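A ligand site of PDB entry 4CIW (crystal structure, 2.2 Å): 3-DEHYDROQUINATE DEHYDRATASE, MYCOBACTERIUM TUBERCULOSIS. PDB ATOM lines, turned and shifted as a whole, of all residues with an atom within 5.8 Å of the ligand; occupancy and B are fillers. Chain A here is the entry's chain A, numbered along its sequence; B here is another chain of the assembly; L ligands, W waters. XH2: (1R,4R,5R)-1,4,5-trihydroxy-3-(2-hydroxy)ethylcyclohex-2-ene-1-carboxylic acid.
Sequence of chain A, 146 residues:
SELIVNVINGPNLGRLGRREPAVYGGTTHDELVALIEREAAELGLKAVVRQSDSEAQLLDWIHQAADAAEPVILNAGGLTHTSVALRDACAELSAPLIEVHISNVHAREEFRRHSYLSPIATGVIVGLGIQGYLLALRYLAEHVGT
The backbone NH (N) of Gly 78 lies within hydrogen-bond range of an oxygen (OAF) of the ligand (3.0 Å). The side-chain hydroxyl (OG) of Ser 103 is in hydrogen-bond range of an oxygen (OAN) of the ligand (2.6 Å). An oxygen (OAM) of the ligand sits at hydrogen-bond distance from the side-chain amide oxygen (OD1) of Asn 75, at 2.8 Å. An oxygen (OAN) of the ligand lies within hydrogen-bond range of the backbone NH (N) of Ser 103 (2.8 Å). OAG of the ligand is in hydrogen-bond range of NE2 of His 81, at 2.7 Å. An oxygen (OAF) of the ligand lies within hydrogen-bond range of the side-chain carboxylate (OD2) of Asp 88 of chain B (2.6 Å). A ring nitrogen (ND1) of His 101 is in hydrogen-bond range of an oxygen (OAM) of the ligand. An oxygen (OAG) of the ligand sits at hydrogen-bond distance from the guanidinium group (NH1) of Arg 112, at 3.0 Å. An oxygen (OAO) of the ligand lies within hydrogen-bond range of the backbone NH of Ile 102 (2.8 Å).
The backbone carbonyl oxygen of Ala 85 of chain B is in hydrogen-bond range of the side-chain amide nitrogen of Asn 12. The guanidinium group of Arg 108 is in hydrogen-bond range of the side-chain hydroxyl of Tyr 24 (3.1 Å). OD1 of Asn 75 lies within hydrogen-bond range of N of Gly 77 (3.1 Å). The side-chain hydroxyl of Tyr 133 lies within hydrogen-bond range of the side-chain amide nitrogen of Asn 75 (3.0 Å). NH2 of Arg 112 lies within salt-bridge range of OD1 of Asp 88 of chain B (2.6 Å). OD1 of Asn 75 lies close to O of Val 100 (3.4 Å). The side-chain hydroxyl of Thr 80 lies within hydrogen-bond range of the backbone carbonyl oxygen of Gly 77, 2.7 Å away. The side-chain hydroxyl (OG) of Ser 103 is in hydrogen-bond range of the guanidinium group (NH1) of Arg 108 (3.0 Å).
Merely in contact with the ligand: Asn 12 (3.5 Å), Tyr 24 (3.4 Å), Gly 77 (3.2 Å) and Val 105 (3.7 Å). 12 residues have an atom within 4 Å of the ligand: Asn 12, Tyr 24, Asn 75, Gly 77, Gly 78, His 81, His 101, Ile 102, Ser 103, Val 105, Arg 112 and Asp 88 of chain B.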
ATOM      1  N   PRO A  11      35.063  28.642 -19.052  1.00  0.00           N
ATOM      2  CA  PRO A  11      35.023  30.038 -18.667  1.00  0.00           C
ATOM      3  C   PRO A  11      33.644  30.607 -18.529  1.00  0.00           C
ATOM      4  O   PRO A  11      32.802  30.331 -19.359  1.00  0.00           O
ATOM      5  CB  PRO A  11      35.728  30.743 -19.809  1.00  0.00           C
ATOM      6  CG  PRO A  11      36.657  29.734 -20.320  1.00  0.00           C
ATOM      7  CD  PRO A  11      35.959  28.432 -20.197  1.00  0.00           C
ATOM      8  N   ASN A  12      33.470  31.367 -17.458  1.00  0.00           N
ATOM      9  CA  ASN A  12      32.266  32.120 -17.127  1.00  0.00           C
ATOM     10  C   ASN A  12      31.133  31.315 -16.574  1.00  0.00           C
ATOM     11  O   ASN A  12      30.131  31.907 -16.165  1.00  0.00           O
ATOM     12  CB  ASN A  12      31.809  32.999 -18.284  1.00  0.00           C
ATOM     13  CG  ASN A  12      32.809  34.066 -18.626  1.00  0.00           C
ATOM     14  OD1 ASN A  12      33.257  34.807 -17.747  1.00  0.00           O
ATOM     15  ND2 ASN A  12      33.193  34.129 -19.888  1.00  0.00           N
ATOM     16  N   LEU A  13      31.291  29.992 -16.512  1.00  0.00           N
ATOM     17  CA  LEU A  13      30.200  29.140 -16.024  1.00  0.00           C
ATOM     18  C   LEU A  13      30.061  29.241 -14.530  1.00  0.00           C
ATOM     19  O   LEU A  13      28.973  28.958 -13.978  1.00  0.00           O
ATOM     20  CB  LEU A  13      30.353  27.678 -16.436  1.00  0.00           C
ATOM     21  CG  LEU A  13      29.730  27.198 -17.767  1.00  0.00           C
ATOM     22  CD1 LEU A  13      28.253  27.577 -17.866  1.00  0.00           C
ATOM     23  CD2 LEU A  13      30.451  27.712 -18.985  1.00  0.00           C
ATOM     24  N   ARG A  15      29.756  31.994 -13.206  1.00  0.00           N
ATOM     25  CA  ARG A  15      28.887  33.146 -13.129  1.00  0.00           C
ATOM     26  C   ARG A  15      27.397  32.829 -13.376  1.00  0.00           C
ATOM     27  O   ARG A  15      26.590  33.748 -13.447  1.00  0.00           O
ATOM     28  CB  ARG A  15      29.317  34.199 -14.145  1.00  0.00           C
ATOM     29  CG  ARG A  15      30.794  34.563 -14.075  1.00  0.00           C
ATOM     30  CD  ARG A  15      31.111  35.360 -12.808  1.00  0.00           C
ATOM     31  NE  ARG A  15      30.417  36.648 -12.886  1.00  0.00           N
ATOM     32  CZ  ARG A  15      30.365  37.556 -11.910  1.00  0.00           C
ATOM     33  NH1 ARG A  15      30.970  37.318 -10.746  1.00  0.00           N
ATOM     34  NH2 ARG A  15      29.709  38.702 -12.112  1.00  0.00           N
ATOM     35  N   TYR A  24      20.834  32.279 -19.578  1.00  0.00           N
ATOM     36  CA  TYR A  24      21.365  31.019 -19.040  1.00  0.00           C
ATOM     37  C   TYR A  24      20.527  30.389 -17.905  1.00  0.00           C
ATOM     38  O   TYR A  24      20.947  29.382 -17.340  1.00  0.00           O
ATOM     39  CB  TYR A  24      22.822  31.213 -18.561  1.00  0.00           C
ATOM     40  CG  TYR A  24      23.812  31.642 -19.621  1.00  0.00           C
ATOM     41  CD1 TYR A  24      24.139  30.807 -20.673  1.00  0.00           C
ATOM     42  CD2 TYR A  24      24.429  32.915 -19.565  1.00  0.00           C
ATOM     43  CE1 TYR A  24      25.053  31.205 -21.662  1.00  0.00           C
ATOM     44  CE2 TYR A  24      25.347  33.328 -20.541  1.00  0.00           C
ATOM     45  CZ  TYR A  24      25.662  32.467 -21.592  1.00  0.00           C
ATOM     46  OH  TYR A  24      26.569  32.845 -22.586  1.00  0.00           O
ATOM     47  N   ASN A  75      30.882  21.481 -20.875  1.00  0.00           N
ATOM     48  CA  ASN A  75      30.392  22.733 -21.369  1.00  0.00           C
ATOM     49  C   ASN A  75      31.550  23.704 -21.309  1.00  0.00           C
ATOM     50  O   ASN A  75      31.911  24.235 -20.224  1.00  0.00           O
ATOM     51  CB  ASN A  75      29.241  23.245 -20.516  1.00  0.00           C
ATOM     52  CG  ASN A  75      28.743  24.587 -21.003  1.00  0.00           C
ATOM     53  OD1 ASN A  75      29.379  25.250 -21.860  1.00  0.00           O
ATOM     54  ND2 ASN A  75      27.613  25.012 -20.461  1.00  0.00           N
ATOM     55  N   ALA A  76      32.193  23.901 -22.449  1.00  0.00           N
ATOM     56  CA  ALA A  76      33.445  24.683 -22.502  1.00  0.00           C
ATOM     57  C   ALA A  76      33.301  26.204 -22.506  1.00  0.00           C
ATOM     58  O   ALA A  76      34.324  26.939 -22.573  1.00  0.00           O
ATOM     59  CB  ALA A  76      34.225  24.254 -23.736  1.00  0.00           C
ATOM     60  N   GLY A  77      32.068  26.717 -22.463  1.00  0.00           N
ATOM     61  CA  GLY A  77      31.796  28.150 -22.550  1.00  0.00           C
ATOM     62  C   GLY A  77      32.328  28.678 -23.879  1.00  0.00           C
ATOM     63  O   GLY A  77      32.173  28.013 -24.903  1.00  0.00           O
ATOM     64  N   GLY A  78      32.993  29.834 -23.854  1.00  0.00           N
ATOM     65  CA  GLY A  78      33.435  30.503 -25.077  1.00  0.00           C
ATOM     66  C   GLY A  78      34.532  29.743 -25.828  1.00  0.00           C
ATOM     67  O   GLY A  78      34.709  29.916 -27.059  1.00  0.00           O
ATOM     68  N   LEU A  79      35.259  28.876 -25.095  1.00  0.00           N
ATOM     69  CA  LEU A  79      36.316  28.083 -25.703  1.00  0.00           C
ATOM     70  C   LEU A  79      35.787  27.051 -26.704  1.00  0.00           C
ATOM     71  O   LEU A  79      36.536  26.548 -27.547  1.00  0.00           O
ATOM     72  CB  LEU A  79      37.108  27.358 -24.638  1.00  0.00           C
ATOM     73  CG  LEU A  79      37.778  28.194 -23.550  1.00  0.00           C
ATOM     74  CD1 LEU A  79      38.513  27.301 -22.587  1.00  0.00           C
ATOM     75  CD2 LEU A  79      38.771  29.166 -24.156  1.00  0.00           C
ATOM     76  N   THR A  80      34.497  26.709 -26.596  1.00  0.00           N
ATOM     77  CA  THR A  80      33.833  25.862 -27.594  1.00  0.00           C
ATOM     78  C   THR A  80      34.133  26.347 -29.004  1.00  0.00           C
ATOM     79  O   THR A  80      34.382  25.564 -29.926  1.00  0.00           O
ATOM     80  CB  THR A  80      32.313  25.918 -27.366  1.00  0.00           C
ATOM     81  OG1 THR A  80      32.016  25.567 -26.006  1.00  0.00           O
ATOM     82  CG2 THR A  80      31.555  24.993 -28.297  1.00  0.00           C
ATOM     83  N   HIS A  81      34.098  27.662 -29.166  1.00  0.00           N
ATOM     84  CA  HIS A  81      34.115  28.262 -30.502  1.00  0.00           C
ATOM     85  C   HIS A  81      35.505  28.645 -30.932  1.00  0.00           C
ATOM     86  O   HIS A  81      35.672  29.022 -32.089  1.00  0.00           O
ATOM     87  CB  HIS A  81      33.225  29.509 -30.531  1.00  0.00           C
ATOM     88  CG  HIS A  81      31.960  29.350 -29.784  1.00  0.00           C
ATOM     89  ND1 HIS A  81      30.983  28.454 -30.164  1.00  0.00           N
ATOM     90  CD2 HIS A  81      31.513  29.927 -28.649  1.00  0.00           C
ATOM     91  CE1 HIS A  81      29.986  28.496 -29.296  1.00  0.00           C
ATOM     92  NE2 HIS A  81      30.282  29.377 -28.373  1.00  0.00           N
ATOM     93  N   VAL A 100      27.620  20.047 -23.955  1.00  0.00           N
ATOM     94  CA  VAL A 100      26.385  20.626 -23.442  1.00  0.00           C
ATOM     95  C   VAL A 100      26.502  22.135 -23.526  1.00  0.00           C
ATOM     96  O   VAL A 100      27.538  22.676 -23.181  1.00  0.00           O
ATOM     97  CB  VAL A 100      26.139  20.199 -21.973  1.00  0.00           C
ATOM     98  CG1 VAL A 100      25.003  21.015 -21.325  1.00  0.00           C
ATOM     99  CG2 VAL A 100      25.767  18.723 -21.928  1.00  0.00           C
ATOM    100  N   HIS A 101      25.454  22.781 -24.029  1.00  0.00           N
ATOM    101  CA  HIS A 101      25.261  24.224 -23.928  1.00  0.00           C
ATOM    102  C   HIS A 101      23.920  24.471 -23.296  1.00  0.00           C
ATOM    103  O   HIS A 101      22.899  23.894 -23.712  1.00  0.00           O
ATOM    104  CB  HIS A 101      25.365  24.908 -25.290  1.00  0.00           C
ATOM    105  CG  HIS A 101      26.694  24.682 -25.928  1.00  0.00           C
ATOM    106  ND1 HIS A 101      27.858  25.225 -25.428  1.00  0.00           N
ATOM    107  CD2 HIS A 101      27.068  23.853 -26.935  1.00  0.00           C
ATOM    108  CE1 HIS A 101      28.881  24.788 -26.135  1.00  0.00           C
ATOM    109  NE2 HIS A 101      28.433  23.966 -27.059  1.00  0.00           N
ATOM    110  N   ILE A 102      23.921  25.356 -22.306  1.00  0.00           N
ATOM    111  CA  ILE A 102      22.728  25.746 -21.581  1.00  0.00           C
ATOM    112  C   ILE A 102      21.805  26.531 -22.512  1.00  0.00           C
ATOM    113  O   ILE A 102      20.598  26.248 -22.587  1.00  0.00           O
ATOM    114  CB  ILE A 102      23.097  26.580 -20.324  1.00  0.00           C
ATOM    115  CG1 ILE A 102      23.842  25.701 -19.331  1.00  0.00           C
ATOM    116  CG2 ILE A 102      21.865  27.216 -19.645  1.00  0.00           C
ATOM    117  CD1 ILE A 102      24.491  26.515 -18.244  1.00  0.00           C
ATOM    118  N   SER A 103      22.380  27.511 -23.212  1.00  0.00           N
ATOM    119  CA  SER A 103      21.593  28.347 -24.111  1.00  0.00           C
ATOM    120  C   SER A 103      21.517  27.669 -25.468  1.00  0.00           C
ATOM    121  O   SER A 103      22.335  26.801 -25.789  1.00  0.00           O
ATOM    122  CB  SER A 103      22.228  29.744 -24.269  1.00  0.00           C
ATOM    123  OG  SER A 103      23.450  29.705 -25.007  1.00  0.00           O
ATOM    124  N   ASN A 104      20.529  28.065 -26.271  1.00  0.00           N
ATOM    125  CA  ASN A 104      20.478  27.630 -27.669  1.00  0.00           C
ATOM    126  C   ASN A 104      21.398  28.551 -28.462  1.00  0.00           C
ATOM    127  O   ASN A 104      21.012  29.655 -28.868  1.00  0.00           O
ATOM    128  CB  ASN A 104      19.043  27.631 -28.210  1.00  0.00           C
ATOM    129  CG  ASN A 104      18.961  27.121 -29.653  1.00  0.00           C
ATOM    130  OD1 ASN A 104      19.979  26.907 -30.322  1.00  0.00           O
ATOM    131  ND2 ASN A 104      17.735  26.918 -30.130  1.00  0.00           N
ATOM    132  N   VAL A 105      22.631  28.082 -28.650  1.00  0.00           N
ATOM    133  CA  VAL A 105      23.650  28.847 -29.393  1.00  0.00           C
ATOM    134  C   VAL A 105      23.227  29.200 -30.861  1.00  0.00           C
ATOM    135  O   VAL A 105      23.667  30.204 -31.430  1.00  0.00           O
ATOM    136  CB  VAL A 105      25.018  28.158 -29.339  1.00  0.00           C
ATOM    137  CG1 VAL A 105      25.535  28.078 -27.918  1.00  0.00           C
ATOM    138  CG2 VAL A 105      24.986  26.742 -29.916  1.00  0.00           C
ATOM    139  N   ARG A 108      21.609  32.644 -31.372  1.00  0.00           N
ATOM    140  CA  ARG A 108      22.384  33.784 -30.888  1.00  0.00           C
ATOM    141  C   ARG A 108      23.274  34.299 -32.023  1.00  0.00           C
ATOM    142  O   ARG A 108      22.913  34.142 -33.188  1.00  0.00           O
ATOM    143  CB  ARG A 108      23.175  33.336 -29.663  1.00  0.00           C
ATOM    144  CG  ARG A 108      22.241  32.926 -28.530  1.00  0.00           C
ATOM    145  CD  ARG A 108      22.989  32.489 -27.293  1.00  0.00           C
ATOM    146  NE  ARG A 108      23.686  33.604 -26.681  1.00  0.00           N
ATOM    147  CZ  ARG A 108      24.561  33.519 -25.701  1.00  0.00           C
ATOM    148  NH1 ARG A 108      24.888  32.335 -25.155  1.00  0.00           N
ATOM    149  NH2 ARG A 108      25.117  34.632 -25.238  1.00  0.00           N
ATOM    150  N   ARG A 112      28.704  31.682 -32.463  1.00  0.00           N
ATOM    151  CA  ARG A 112      28.358  30.633 -31.505  1.00  0.00           C
ATOM    152  C   ARG A 112      27.836  29.383 -32.158  1.00  0.00           C
ATOM    153  O   ARG A 112      27.727  28.348 -31.492  1.00  0.00           O
ATOM    154  CB  ARG A 112      27.348  31.125 -30.492  1.00  0.00           C
ATOM    155  CG  ARG A 112      27.887  32.251 -29.634  1.00  0.00           C
ATOM    156  CD  ARG A 112      26.959  32.594 -28.451  1.00  0.00           C
ATOM    157  NE  ARG A 112      27.291  33.939 -27.988  1.00  0.00           N
ATOM    158  CZ  ARG A 112      28.242  34.239 -27.105  1.00  0.00           C
ATOM    159  NH1 ARG A 112      28.950  33.264 -26.476  1.00  0.00           N
ATOM    160  NH2 ARG A 112      28.447  35.526 -26.809  1.00  0.00           N
ATOM    161  N   TYR A 133      22.520  18.903 -18.719  1.00  0.00           N
ATOM    162  CA  TYR A 133      23.483  18.098 -17.930  1.00  0.00           C
ATOM    163  C   TYR A 133      22.860  16.787 -17.376  1.00  0.00           C
ATOM    164  O   TYR A 133      23.463  15.723 -17.444  1.00  0.00           O
ATOM    165  CB  TYR A 133      24.021  18.900 -16.738  1.00  0.00           C
ATOM    166  CG  TYR A 133      24.872  20.095 -17.070  1.00  0.00           C
ATOM    167  CD1 TYR A 133      26.259  19.979 -17.226  1.00  0.00           C
ATOM    168  CD2 TYR A 133      24.286  21.361 -17.212  1.00  0.00           C
ATOM    169  CE1 TYR A 133      27.039  21.075 -17.534  1.00  0.00           C
ATOM    170  CE2 TYR A 133      25.057  22.471 -17.502  1.00  0.00           C
ATOM    171  CZ  TYR A 133      26.427  22.338 -17.666  1.00  0.00           C
ATOM    172  OH  TYR A 133      27.171  23.459 -17.963  1.00  0.00           O
ATOM    173  N   VAL B  84      36.027  34.738 -27.239  1.00  0.00           N
ATOM    174  CA  VAL B  84      34.596  34.793 -26.921  1.00  0.00           C
ATOM    175  C   VAL B  84      34.387  34.849 -25.404  1.00  0.00           C
ATOM    176  O   VAL B  84      33.558  35.601 -24.929  1.00  0.00           O
ATOM    177  CB  VAL B  84      33.858  33.593 -27.564  1.00  0.00           C
ATOM    178  CG1 VAL B  84      32.389  33.531 -27.163  1.00  0.00           C
ATOM    179  CG2 VAL B  84      33.970  33.704 -29.082  1.00  0.00           C
ATOM    180  N   ALA B  85      35.193  34.103 -24.646  1.00  0.00           N
ATOM    181  CA  ALA B  85      35.112  34.091 -23.174  1.00  0.00           C
ATOM    182  C   ALA B  85      35.223  35.497 -22.573  1.00  0.00           C
ATOM    183  O   ALA B  85      34.475  35.857 -21.671  1.00  0.00           O
ATOM    184  CB  ALA B  85      36.193  33.180 -22.586  1.00  0.00           C
ATOM    185  N   ASP B  88      32.028  37.348 -23.373  1.00  0.00           N
ATOM    186  CA  ASP B  88      30.968  36.933 -22.453  1.00  0.00           C
ATOM    187  C   ASP B  88      31.073  37.577 -21.049  1.00  0.00           C
ATOM    188  O   ASP B  88      30.056  37.934 -20.453  1.00  0.00           O
ATOM    189  CB  ASP B  88      30.829  35.414 -22.430  1.00  0.00           C
ATOM    190  CG  ASP B  88      30.125  34.876 -23.673  1.00  0.00           C
ATOM    191  OD1 ASP B  88      29.622  35.692 -24.494  1.00  0.00           O
ATOM    192  OD2 ASP B  88      30.072  33.646 -23.855  1.00  0.00           O
HETATM  193  OAF XH2 L   1      30.311  31.129 -24.266  1.00  0.00           O
HETATM  194  CAC XH2 L   1      28.939  30.719 -23.996  1.00  0.00           C
HETATM  195  CAB XH2 L   1      28.630  29.652 -25.088  1.00  0.00           C
HETATM  196  OAG XH2 L   1      28.624  30.280 -26.419  1.00  0.00           O
HETATM  197  CAA XH2 L   1      27.278  29.006 -24.762  1.00  0.00           C
HETATM  198  CAI XH2 L   1      27.399  28.275 -23.401  1.00  0.00           C
HETATM  199  CAH XH2 L   1      26.093  27.810 -22.957  1.00  0.00           C
HETATM  200  OAO XH2 L   1      26.076  27.038 -21.950  1.00  0.00           O
HETATM  201  OAN XH2 L   1      25.048  28.197 -23.594  1.00  0.00           O
HETATM  202  OAM XH2 L   1      28.318  27.134 -23.566  1.00  0.00           O
HETATM  203  CAE XH2 L   1      28.033  29.082 -22.396  1.00  0.00           C
HETATM  204  CAD XH2 L   1      28.777  30.248 -22.620  1.00  0.00           C
HETATM  205  CAL XH2 L   1      29.328  30.975 -21.516  1.00  0.00           C
HETATM  206  CAK XH2 L   1      28.369  30.970 -20.306  1.00  0.00           C
HETATM  207  OAJ XH2 L   1      28.596  32.129 -19.396  1.00  0.00           O
HETATM  208  O   HOH W   1      27.959  35.162 -18.274  1.00  0.00           O
